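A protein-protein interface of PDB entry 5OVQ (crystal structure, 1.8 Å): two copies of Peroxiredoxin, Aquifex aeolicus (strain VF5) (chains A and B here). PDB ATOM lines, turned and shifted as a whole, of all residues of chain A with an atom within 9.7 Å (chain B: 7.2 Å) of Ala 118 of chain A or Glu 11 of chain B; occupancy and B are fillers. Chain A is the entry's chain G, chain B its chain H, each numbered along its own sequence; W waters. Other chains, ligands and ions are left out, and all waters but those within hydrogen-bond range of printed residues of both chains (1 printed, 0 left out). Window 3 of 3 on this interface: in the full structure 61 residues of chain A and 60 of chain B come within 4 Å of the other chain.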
ATOM      1  N   MET A 114     -20.939 -29.424  24.707  1.00  0.00           N
ATOM      2  CA  MET A 114     -21.553 -30.203  23.655  1.00  0.00           C
ATOM      3  C   MET A 114     -23.030 -30.478  23.893  1.00  0.00           C
ATOM      4  O   MET A 114     -23.706 -30.948  22.973  1.00  0.00           O
ATOM      5  CB  MET A 114     -20.805 -31.518  23.487  1.00  0.00           C
ATOM      6  CG  MET A 114     -19.342 -31.394  23.042  1.00  0.00           C
ATOM      7  SD  MET A 114     -18.619 -33.057  23.057  1.00  0.00           S
ATOM      8  CE  MET A 114     -16.948 -32.821  22.481  1.00  0.00           C
ATOM      9  N   ILE A 115     -23.547 -30.191  25.088  1.00  0.00           N
ATOM     10  CA  ILE A 115     -24.943 -30.456  25.426  1.00  0.00           C
ATOM     11  C   ILE A 115     -25.737 -29.162  25.320  1.00  0.00           C
ATOM     12  O   ILE A 115     -25.561 -28.251  26.139  1.00  0.00           O
ATOM     13  CB  ILE A 115     -25.079 -31.061  26.831  1.00  0.00           C
ATOM     14  CG1 ILE A 115     -24.215 -32.318  26.975  1.00  0.00           C
ATOM     15  CG2 ILE A 115     -26.534 -31.371  27.118  1.00  0.00           C
ATOM     16  CD1 ILE A 115     -24.632 -33.465  26.057  1.00  0.00           C
ATOM     17  N   HIS A 116     -26.664 -29.108  24.365  1.00  0.00           N
ATOM     18  CA  HIS A 116     -27.552 -27.957  24.182  1.00  0.00           C
ATOM     19  C   HIS A 116     -28.979 -28.425  24.419  1.00  0.00           C
ATOM     20  O   HIS A 116     -29.565 -29.085  23.546  1.00  0.00           O
ATOM     21  CB  HIS A 116     -27.388 -27.363  22.780  1.00  0.00           C
ATOM     22  CG  HIS A 116     -26.046 -26.743  22.568  1.00  0.00           C
ATOM     23  ND1 HIS A 116     -25.874 -25.385  22.390  1.00  0.00           N
ATOM     24  CD2 HIS A 116     -24.805 -27.285  22.562  1.00  0.00           C
ATOM     25  CE1 HIS A 116     -24.585 -25.125  22.249  1.00  0.00           C
ATOM     26  NE2 HIS A 116     -23.915 -26.259  22.353  1.00  0.00           N
ATOM     27  N   PRO A 117     -29.568 -28.130  25.586  1.00  0.00           N
ATOM     28  CA  PRO A 117     -30.796 -28.843  26.003  1.00  0.00           C
ATOM     29  C   PRO A 117     -31.974 -28.713  25.048  1.00  0.00           C
ATOM     30  O   PRO A 117     -32.760 -29.659  24.931  1.00  0.00           O
ATOM     31  CB  PRO A 117     -31.118 -28.213  27.363  1.00  0.00           C
ATOM     32  CG  PRO A 117     -29.810 -27.694  27.862  1.00  0.00           C
ATOM     33  CD  PRO A 117     -29.053 -27.245  26.644  1.00  0.00           C
ATOM     34  N   ALA A 118     -32.128 -27.579  24.355  1.00  0.00           N
ATOM     35  CA  ALA A 118     -33.212 -27.444  23.386  1.00  0.00           C
ATOM     36  C   ALA A 118     -33.000 -28.339  22.175  1.00  0.00           C
ATOM     37  O   ALA A 118     -33.966 -28.668  21.480  1.00  0.00           O
ATOM     38  CB  ALA A 118     -33.350 -25.985  22.936  1.00  0.00           C
ATOM     39  N   GLN A 119     -31.754 -28.725  21.904  1.00  0.00           N
ATOM     40  CA  GLN A 119     -31.468 -29.749  20.915  1.00  0.00           C
ATOM     41  C   GLN A 119     -31.694 -31.129  21.509  1.00  0.00           C
ATOM     42  O   GLN A 119     -32.449 -31.938  20.960  1.00  0.00           O
ATOM     43  CB  GLN A 119     -30.031 -29.614  20.426  1.00  0.00           C
ATOM     44  CG  GLN A 119     -29.839 -28.467  19.449  1.00  0.00           C
ATOM     45  CD  GLN A 119     -30.073 -28.938  18.026  1.00  0.00           C
ATOM     46  OE1 GLN A 119     -29.225 -29.612  17.446  1.00  0.00           O
ATOM     47  NE2 GLN A 119     -31.245 -28.641  17.481  1.00  0.00           N
ATOM     48  N   SER A 120     -31.049 -31.405  22.641  1.00  0.00           N
ATOM     49  CA  SER A 120     -31.212 -32.672  23.340  1.00  0.00           C
ATOM     50  C   SER A 120     -30.662 -32.503  24.741  1.00  0.00           C
ATOM     51  O   SER A 120     -29.598 -31.904  24.925  1.00  0.00           O
ATOM     52  CB  SER A 120     -30.485 -33.823  22.627  1.00  0.00           C
ATOM     53  OG  SER A 120     -30.543 -35.042  23.371  1.00  0.00           O
ATOM     54  N   THR A 121     -31.386 -33.029  25.724  1.00  0.00           N
ATOM     55  CA  THR A 121     -30.861 -33.106  27.076  1.00  0.00           C
ATOM     56  C   THR A 121     -30.063 -34.385  27.306  1.00  0.00           C
ATOM     57  O   THR A 121     -29.480 -34.551  28.380  1.00  0.00           O
ATOM     58  CB  THR A 121     -31.999 -33.006  28.095  1.00  0.00           C
ATOM     59  OG1 THR A 121     -32.943 -34.056  27.859  1.00  0.00           O
ATOM     60  CG2 THR A 121     -32.700 -31.653  27.959  1.00  0.00           C
ATOM     61  N   THR A 122     -30.010 -35.280  26.324  1.00  0.00           N
ATOM     62  CA  THR A 122     -29.329 -36.558  26.486  1.00  0.00           C
ATOM     63  C   THR A 122     -28.172 -36.801  25.516  1.00  0.00           C
ATOM     64  O   THR A 122     -27.261 -37.560  25.856  1.00  0.00           O
ATOM     65  CB  THR A 122     -30.335 -37.722  26.354  1.00  0.00           C
ATOM     66  OG1 THR A 122     -30.915 -37.719  25.045  1.00  0.00           O
ATOM     67  CG2 THR A 122     -31.447 -37.596  27.395  1.00  0.00           C
ATOM     68  N   PHE A 123     -28.193 -36.218  24.318  1.00  0.00           N
ATOM     69  CA  PHE A 123     -27.171 -36.435  23.302  1.00  0.00           C
ATOM     70  C   PHE A 123     -26.373 -35.154  23.069  1.00  0.00           C
ATOM     71  O   PHE A 123     -26.892 -34.056  23.256  1.00  0.00           O
ATOM     72  CB  PHE A 123     -27.776 -36.849  21.954  1.00  0.00           C
ATOM     73  CG  PHE A 123     -28.777 -37.962  22.025  1.00  0.00           C
ATOM     74  CD1 PHE A 123     -28.552 -39.090  22.793  1.00  0.00           C
ATOM     75  CD2 PHE A 123     -29.927 -37.898  21.249  1.00  0.00           C
ATOM     76  CE1 PHE A 123     -29.478 -40.122  22.819  1.00  0.00           C
ATOM     77  CE2 PHE A 123     -30.851 -38.923  21.264  1.00  0.00           C
ATOM     78  CZ  PHE A 123     -30.629 -40.037  22.057  1.00  0.00           C
ATOM     79  N   VAL A 125     -24.630 -32.391  20.530  1.00  0.00           N
ATOM     80  CA  VAL A 125     -24.833 -31.852  19.189  1.00  0.00           C
ATOM     81  C   VAL A 125     -23.636 -32.276  18.347  1.00  0.00           C
ATOM     82  O   VAL A 125     -22.799 -33.075  18.794  1.00  0.00           O
ATOM     83  CB  VAL A 125     -25.015 -30.322  19.217  1.00  0.00           C
ATOM     84  CG1 VAL A 125     -26.235 -29.955  20.065  1.00  0.00           C
ATOM     85  CG2 VAL A 125     -23.770 -29.646  19.788  1.00  0.00           C
ATOM     86  N   PRO A 144     -26.172 -28.553  14.355  1.00  0.00           N
ATOM     87  CA  PRO A 144     -27.289 -29.168  15.078  1.00  0.00           C
ATOM     88  C   PRO A 144     -27.489 -30.621  14.643  1.00  0.00           C
ATOM     89  O   PRO A 144     -26.848 -31.125  13.717  1.00  0.00           O
ATOM     90  CB  PRO A 144     -28.478 -28.290  14.682  1.00  0.00           C
ATOM     91  CG  PRO A 144     -28.127 -27.841  13.281  1.00  0.00           C
ATOM     92  CD  PRO A 144     -26.635 -27.622  13.306  1.00  0.00           C
ATOM     93  N   LEU A 145     -28.427 -31.287  15.326  1.00  0.00           N
ATOM     94  CA  LEU A 145     -28.655 -32.708  15.084  1.00  0.00           C
ATOM     95  C   LEU A 145     -29.057 -32.979  13.644  1.00  0.00           C
ATOM     96  O   LEU A 145     -28.735 -34.041  13.095  1.00  0.00           O
ATOM     97  CB  LEU A 145     -29.740 -33.229  16.024  1.00  0.00           C
ATOM     98  CG  LEU A 145     -29.495 -33.037  17.517  1.00  0.00           C
ATOM     99  CD1 LEU A 145     -30.662 -33.629  18.295  1.00  0.00           C
ATOM    100  CD2 LEU A 145     -28.179 -33.675  17.914  1.00  0.00           C
ATOM    101  N   PRO B   7     -23.555 -19.664  23.578  1.00  0.00           N
ATOM    102  CA  PRO B   7     -24.921 -19.512  23.074  1.00  0.00           C
ATOM    103  C   PRO B   7     -25.513 -20.891  22.826  1.00  0.00           C
ATOM    104  O   PRO B   7     -24.815 -21.826  22.422  1.00  0.00           O
ATOM    105  CB  PRO B   7     -24.743 -18.713  21.779  1.00  0.00           C
ATOM    106  CG  PRO B   7     -23.404 -18.069  21.914  1.00  0.00           C
ATOM    107  CD  PRO B   7     -22.571 -19.050  22.674  1.00  0.00           C
ATOM    108  N   ARG B   8     -26.811 -21.022  23.068  1.00  0.00           N
ATOM    109  CA  ARG B   8     -27.449 -22.334  23.086  1.00  0.00           C
ATOM    110  C   ARG B   8     -28.187 -22.585  21.775  1.00  0.00           C
ATOM    111  O   ARG B   8     -29.064 -21.802  21.391  1.00  0.00           O
ATOM    112  CB  ARG B   8     -28.410 -22.462  24.263  1.00  0.00           C
ATOM    113  CG  ARG B   8     -27.717 -22.388  25.621  1.00  0.00           C
ATOM    114  CD  ARG B   8     -28.719 -22.619  26.716  1.00  0.00           C
ATOM    115  NE  ARG B   8     -28.123 -22.676  28.042  1.00  0.00           N
ATOM    116  CZ  ARG B   8     -28.769 -23.116  29.115  1.00  0.00           C
ATOM    117  NH1 ARG B   8     -30.017 -23.551  28.999  1.00  0.00           N
ATOM    118  NH2 ARG B   8     -28.168 -23.134  30.296  1.00  0.00           N
ATOM    119  N   LEU B   9     -27.831 -23.676  21.099  1.00  0.00           N
ATOM    120  CA  LEU B   9     -28.523 -24.087  19.880  1.00  0.00           C
ATOM    121  C   LEU B   9     -29.972 -24.465  20.184  1.00  0.00           C
ATOM    122  O   LEU B   9     -30.266 -25.127  21.181  1.00  0.00           O
ATOM    123  CB  LEU B   9     -27.788 -25.266  19.241  1.00  0.00           C
ATOM    124  CG  LEU B   9     -26.357 -25.024  18.757  1.00  0.00           C
ATOM    125  CD1 LEU B   9     -25.809 -26.298  18.117  1.00  0.00           C
ATOM    126  CD2 LEU B   9     -26.309 -23.860  17.734  1.00  0.00           C
ATOM    127  N   GLY B  10     -30.887 -24.033  19.316  1.00  0.00           N
ATOM    128  CA  GLY B  10     -32.296 -24.336  19.466  1.00  0.00           C
ATOM    129  C   GLY B  10     -33.078 -23.381  20.337  1.00  0.00           C
ATOM    130  O   GLY B  10     -34.291 -23.566  20.498  1.00  0.00           O
ATOM    131  N   GLU B  11     -32.433 -22.364  20.894  1.00  0.00           N
ATOM    132  CA  GLU B  11     -33.048 -21.340  21.722  1.00  0.00           C
ATOM    133  C   GLU B  11     -32.983 -19.993  21.022  1.00  0.00           C
ATOM    134  O   GLU B  11     -32.150 -19.796  20.131  1.00  0.00           O
ATOM    135  CB  GLU B  11     -32.340 -21.270  23.081  1.00  0.00           C
ATOM    136  CG  GLU B  11     -32.473 -22.593  23.849  1.00  0.00           C
ATOM    137  CD  GLU B  11     -31.830 -22.584  25.221  1.00  0.00           C
ATOM    138  OE1 GLU B  11     -31.784 -21.516  25.871  1.00  0.00           O
ATOM    139  OE2 GLU B  11     -31.366 -23.658  25.647  1.00  0.00           O
ATOM    140  N   PRO B  12     -33.854 -19.046  21.383  1.00  0.00           N
ATOM    141  CA  PRO B  12     -33.806 -17.725  20.745  1.00  0.00           C
ATOM    142  C   PRO B  12     -32.404 -17.145  20.806  1.00  0.00           C
ATOM    143  O   PRO B  12     -31.711 -17.244  21.825  1.00  0.00           O
ATOM    144  CB  PRO B  12     -34.797 -16.900  21.569  1.00  0.00           C
ATOM    145  CG  PRO B  12     -35.771 -17.889  22.066  1.00  0.00           C
ATOM    146  CD  PRO B  12     -34.989 -19.157  22.314  1.00  0.00           C
ATOM    147  N   ALA B  13     -31.983 -16.552  19.697  1.00  0.00           N
ATOM    148  CA  ALA B  13     -30.688 -15.905  19.663  1.00  0.00           C
ATOM    149  C   ALA B  13     -30.669 -14.744  20.655  1.00  0.00           C
ATOM    150  O   ALA B  13     -31.667 -14.020  20.783  1.00  0.00           O
ATOM    151  CB  ALA B  13     -30.376 -15.406  18.252  1.00  0.00           C
ATOM    152  N   PRO B  14     -29.570 -14.546  21.377  1.00  0.00           N
ATOM    153  CA  PRO B  14     -29.509 -13.456  22.364  1.00  0.00           C
ATOM    154  C   PRO B  14     -29.919 -12.114  21.765  1.00  0.00           C
ATOM    155  O   PRO B  14     -29.401 -11.688  20.728  1.00  0.00           O
ATOM    156  CB  PRO B  14     -28.040 -13.464  22.796  1.00  0.00           C
ATOM    157  CG  PRO B  14     -27.615 -14.895  22.610  1.00  0.00           C
ATOM    158  CD  PRO B  14     -28.348 -15.370  21.379  1.00  0.00           C
ATOM    159  N   ILE B 131     -29.155 -18.106  12.168  1.00  0.00           N
ATOM    160  CA  ILE B 131     -30.374 -17.880  12.927  1.00  0.00           C
ATOM    161  C   ILE B 131     -31.533 -17.970  11.954  1.00  0.00           C
ATOM    162  O   ILE B 131     -31.447 -17.464  10.831  1.00  0.00           O
ATOM    163  CB  ILE B 131     -30.346 -16.516  13.642  1.00  0.00           C
ATOM    164  CG1 ILE B 131     -29.247 -16.510  14.705  1.00  0.00           C
ATOM    165  CG2 ILE B 131     -31.714 -16.155  14.196  1.00  0.00           C
ATOM    166  CD1 ILE B 131     -28.756 -15.109  15.089  1.00  0.00           C
ATOM    167  N   GLY B 135     -35.981 -16.435  14.745  1.00  0.00           N
ATOM    168  CA  GLY B 135     -35.009 -15.944  15.700  1.00  0.00           C
ATOM    169  C   GLY B 135     -34.285 -17.010  16.491  1.00  0.00           C
ATOM    170  O   GLY B 135     -33.640 -16.683  17.493  1.00  0.00           O
ATOM    171  N   ILE B 136     -34.362 -18.271  16.077  1.00  0.00           N
ATOM    172  CA  ILE B 136     -33.759 -19.371  16.822  1.00  0.00           C
ATOM    173  C   ILE B 136     -32.336 -19.598  16.324  1.00  0.00           C
ATOM    174  O   ILE B 136     -32.091 -19.677  15.114  1.00  0.00           O
ATOM    175  CB  ILE B 136     -34.613 -20.642  16.688  1.00  0.00           C
ATOM    176  CG1 ILE B 136     -36.022 -20.388  17.244  1.00  0.00           C
ATOM    177  CG2 ILE B 136     -33.945 -21.837  17.366  1.00  0.00           C
ATOM    178  CD1 ILE B 136     -36.079 -20.076  18.736  1.00  0.00           C
ATOM    179  N   LEU B 137     -31.395 -19.718  17.259  1.00  0.00           N
ATOM    180  CA  LEU B 137     -30.021 -20.046  16.905  1.00  0.00           C
ATOM    181  C   LEU B 137     -29.966 -21.485  16.414  1.00  0.00           C
ATOM    182  O   LEU B 137     -30.412 -22.398  17.108  1.00  0.00           O
ATOM    183  CB  LEU B 137     -29.098 -19.855  18.108  1.00  0.00           C
ATOM    184  CG  LEU B 137     -27.636 -20.223  17.849  1.00  0.00           C
ATOM    185  CD1 LEU B 137     -27.061 -19.337  16.714  1.00  0.00           C
ATOM    186  CD2 LEU B 137     -26.817 -20.066  19.116  1.00  0.00           C
ATOM    187  N   ARG B 138     -29.435 -21.688  15.211  1.00  0.00           N
ATOM    188  CA  ARG B 138     -29.470 -23.002  14.585  1.00  0.00           C
ATOM    189  C   ARG B 138     -28.112 -23.670  14.488  1.00  0.00           C
ATOM    190  O   ARG B 138     -28.036 -24.893  14.560  1.00  0.00           O
ATOM    191  CB  ARG B 138     -30.068 -22.901  13.181  1.00  0.00           C
ATOM    192  CG  ARG B 138     -31.462 -22.306  13.148  1.00  0.00           C
ATOM    193  CD  ARG B 138     -32.434 -23.203  13.882  1.00  0.00           C
ATOM    194  NE  ARG B 138     -32.531 -24.497  13.214  1.00  0.00           N
ATOM    195  CZ  ARG B 138     -33.406 -24.779  12.254  1.00  0.00           C
ATOM    196  NH1 ARG B 138     -34.282 -23.865  11.852  1.00  0.00           N
ATOM    197  NH2 ARG B 138     -33.413 -25.986  11.709  1.00  0.00           N
HETATM  198  O   HOH W   1     -30.082 -25.531  24.060  1.00  0.00           O
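NH1 of Arg 8 of chain B lies within salt-bridge range of OE2 of Glu 11 of chain B. OE1 of Gln 119 of chain A sits at hydrogen-bond distance from N of Leu 145 of chain A, 2.8 Å away. O of Glu 11 of chain B is in hydrogen-bond range of N of Leu 137 of chain B (3.0 Å). O of Leu 137 of chain B lies within hydrogen-bond range of N of Gly 10 of chain B (2.8 Å).
Of the 13 printed residues of chain B, 6 touch a printed residue of chain A. Hydrophobic or aromatic side chains of chain A within 4 Å of the printed part of chain B: His 116, Ala 118 and Pro 144. Among the printed residues, no Asp or Glu carboxylate lies within 4 Å of a Lys or Arg side-chain nitrogen of the other chain.
His 116 of chain A touches Pro 7 of chain B (CE1 to O, 3.3 Å). His 116 of chain A touches Arg 8 of chain B (ND1 to CA, 3.5 Å). Leu 9 of chain B touches Ala 118 of chain A. Gly 10 of chain B touches Ala 118 of chain A (O to CB, 3.6 Å). Ala 118 of chain A touches Glu 11 of chain B (CB to CG, 3.6 Å). Leu 9 of chain B touches Gln 119 of chain A (O to CG, 3.8 Å). Arg 138 of chain B touches Pro 144 of chain A.
A ring nitrogen (ND1) of His 116 of chain A lies within hydrogen-bond range of the backbone NH (N) of Leu 9 of chain B.
No position is printed for both chains. Of the 8 pairs that touch across the chains among the printed residues, none has its exchanged pair printed and touching as well.
Of the printed residues of chain B, His 116 of chain A touches Pro 7, Arg 8 and Leu 9. Of the printed residues of chain B, Pro 144 of chain A touches Arg 138. Of the printed residues of chain A, Arg 8 of chain B touches His 116 (3.5 Å). Printed residues of chain A within 4 Å of Leu 9 of chain B: His 116, Ala 118 and Gln 119. Of chain A, only Ala 118 comes within 4 Å of Gly 10 of chain B. Glu 11 of chain B touches just one residue of chain A: Ala 118. The nearest residue of chain B that does not touch Ala 118 of chain A is Arg 8 of chain B (6.2 Å). The nearest printed residue of chain B that does not touch Gln 119 of chain A is Gly 10 of chain B (4.6 Å).
Water W1 lies within hydrogen-bond range of the side-chain carboxylate (OE2) of Glu 11 of chain B (2.8 Å), the backbone NH (N) of Ala 118 of chain A (2.9 Å) and the backbone carbonyl oxygen (O) of Leu 9 of chain B (2.9 Å).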
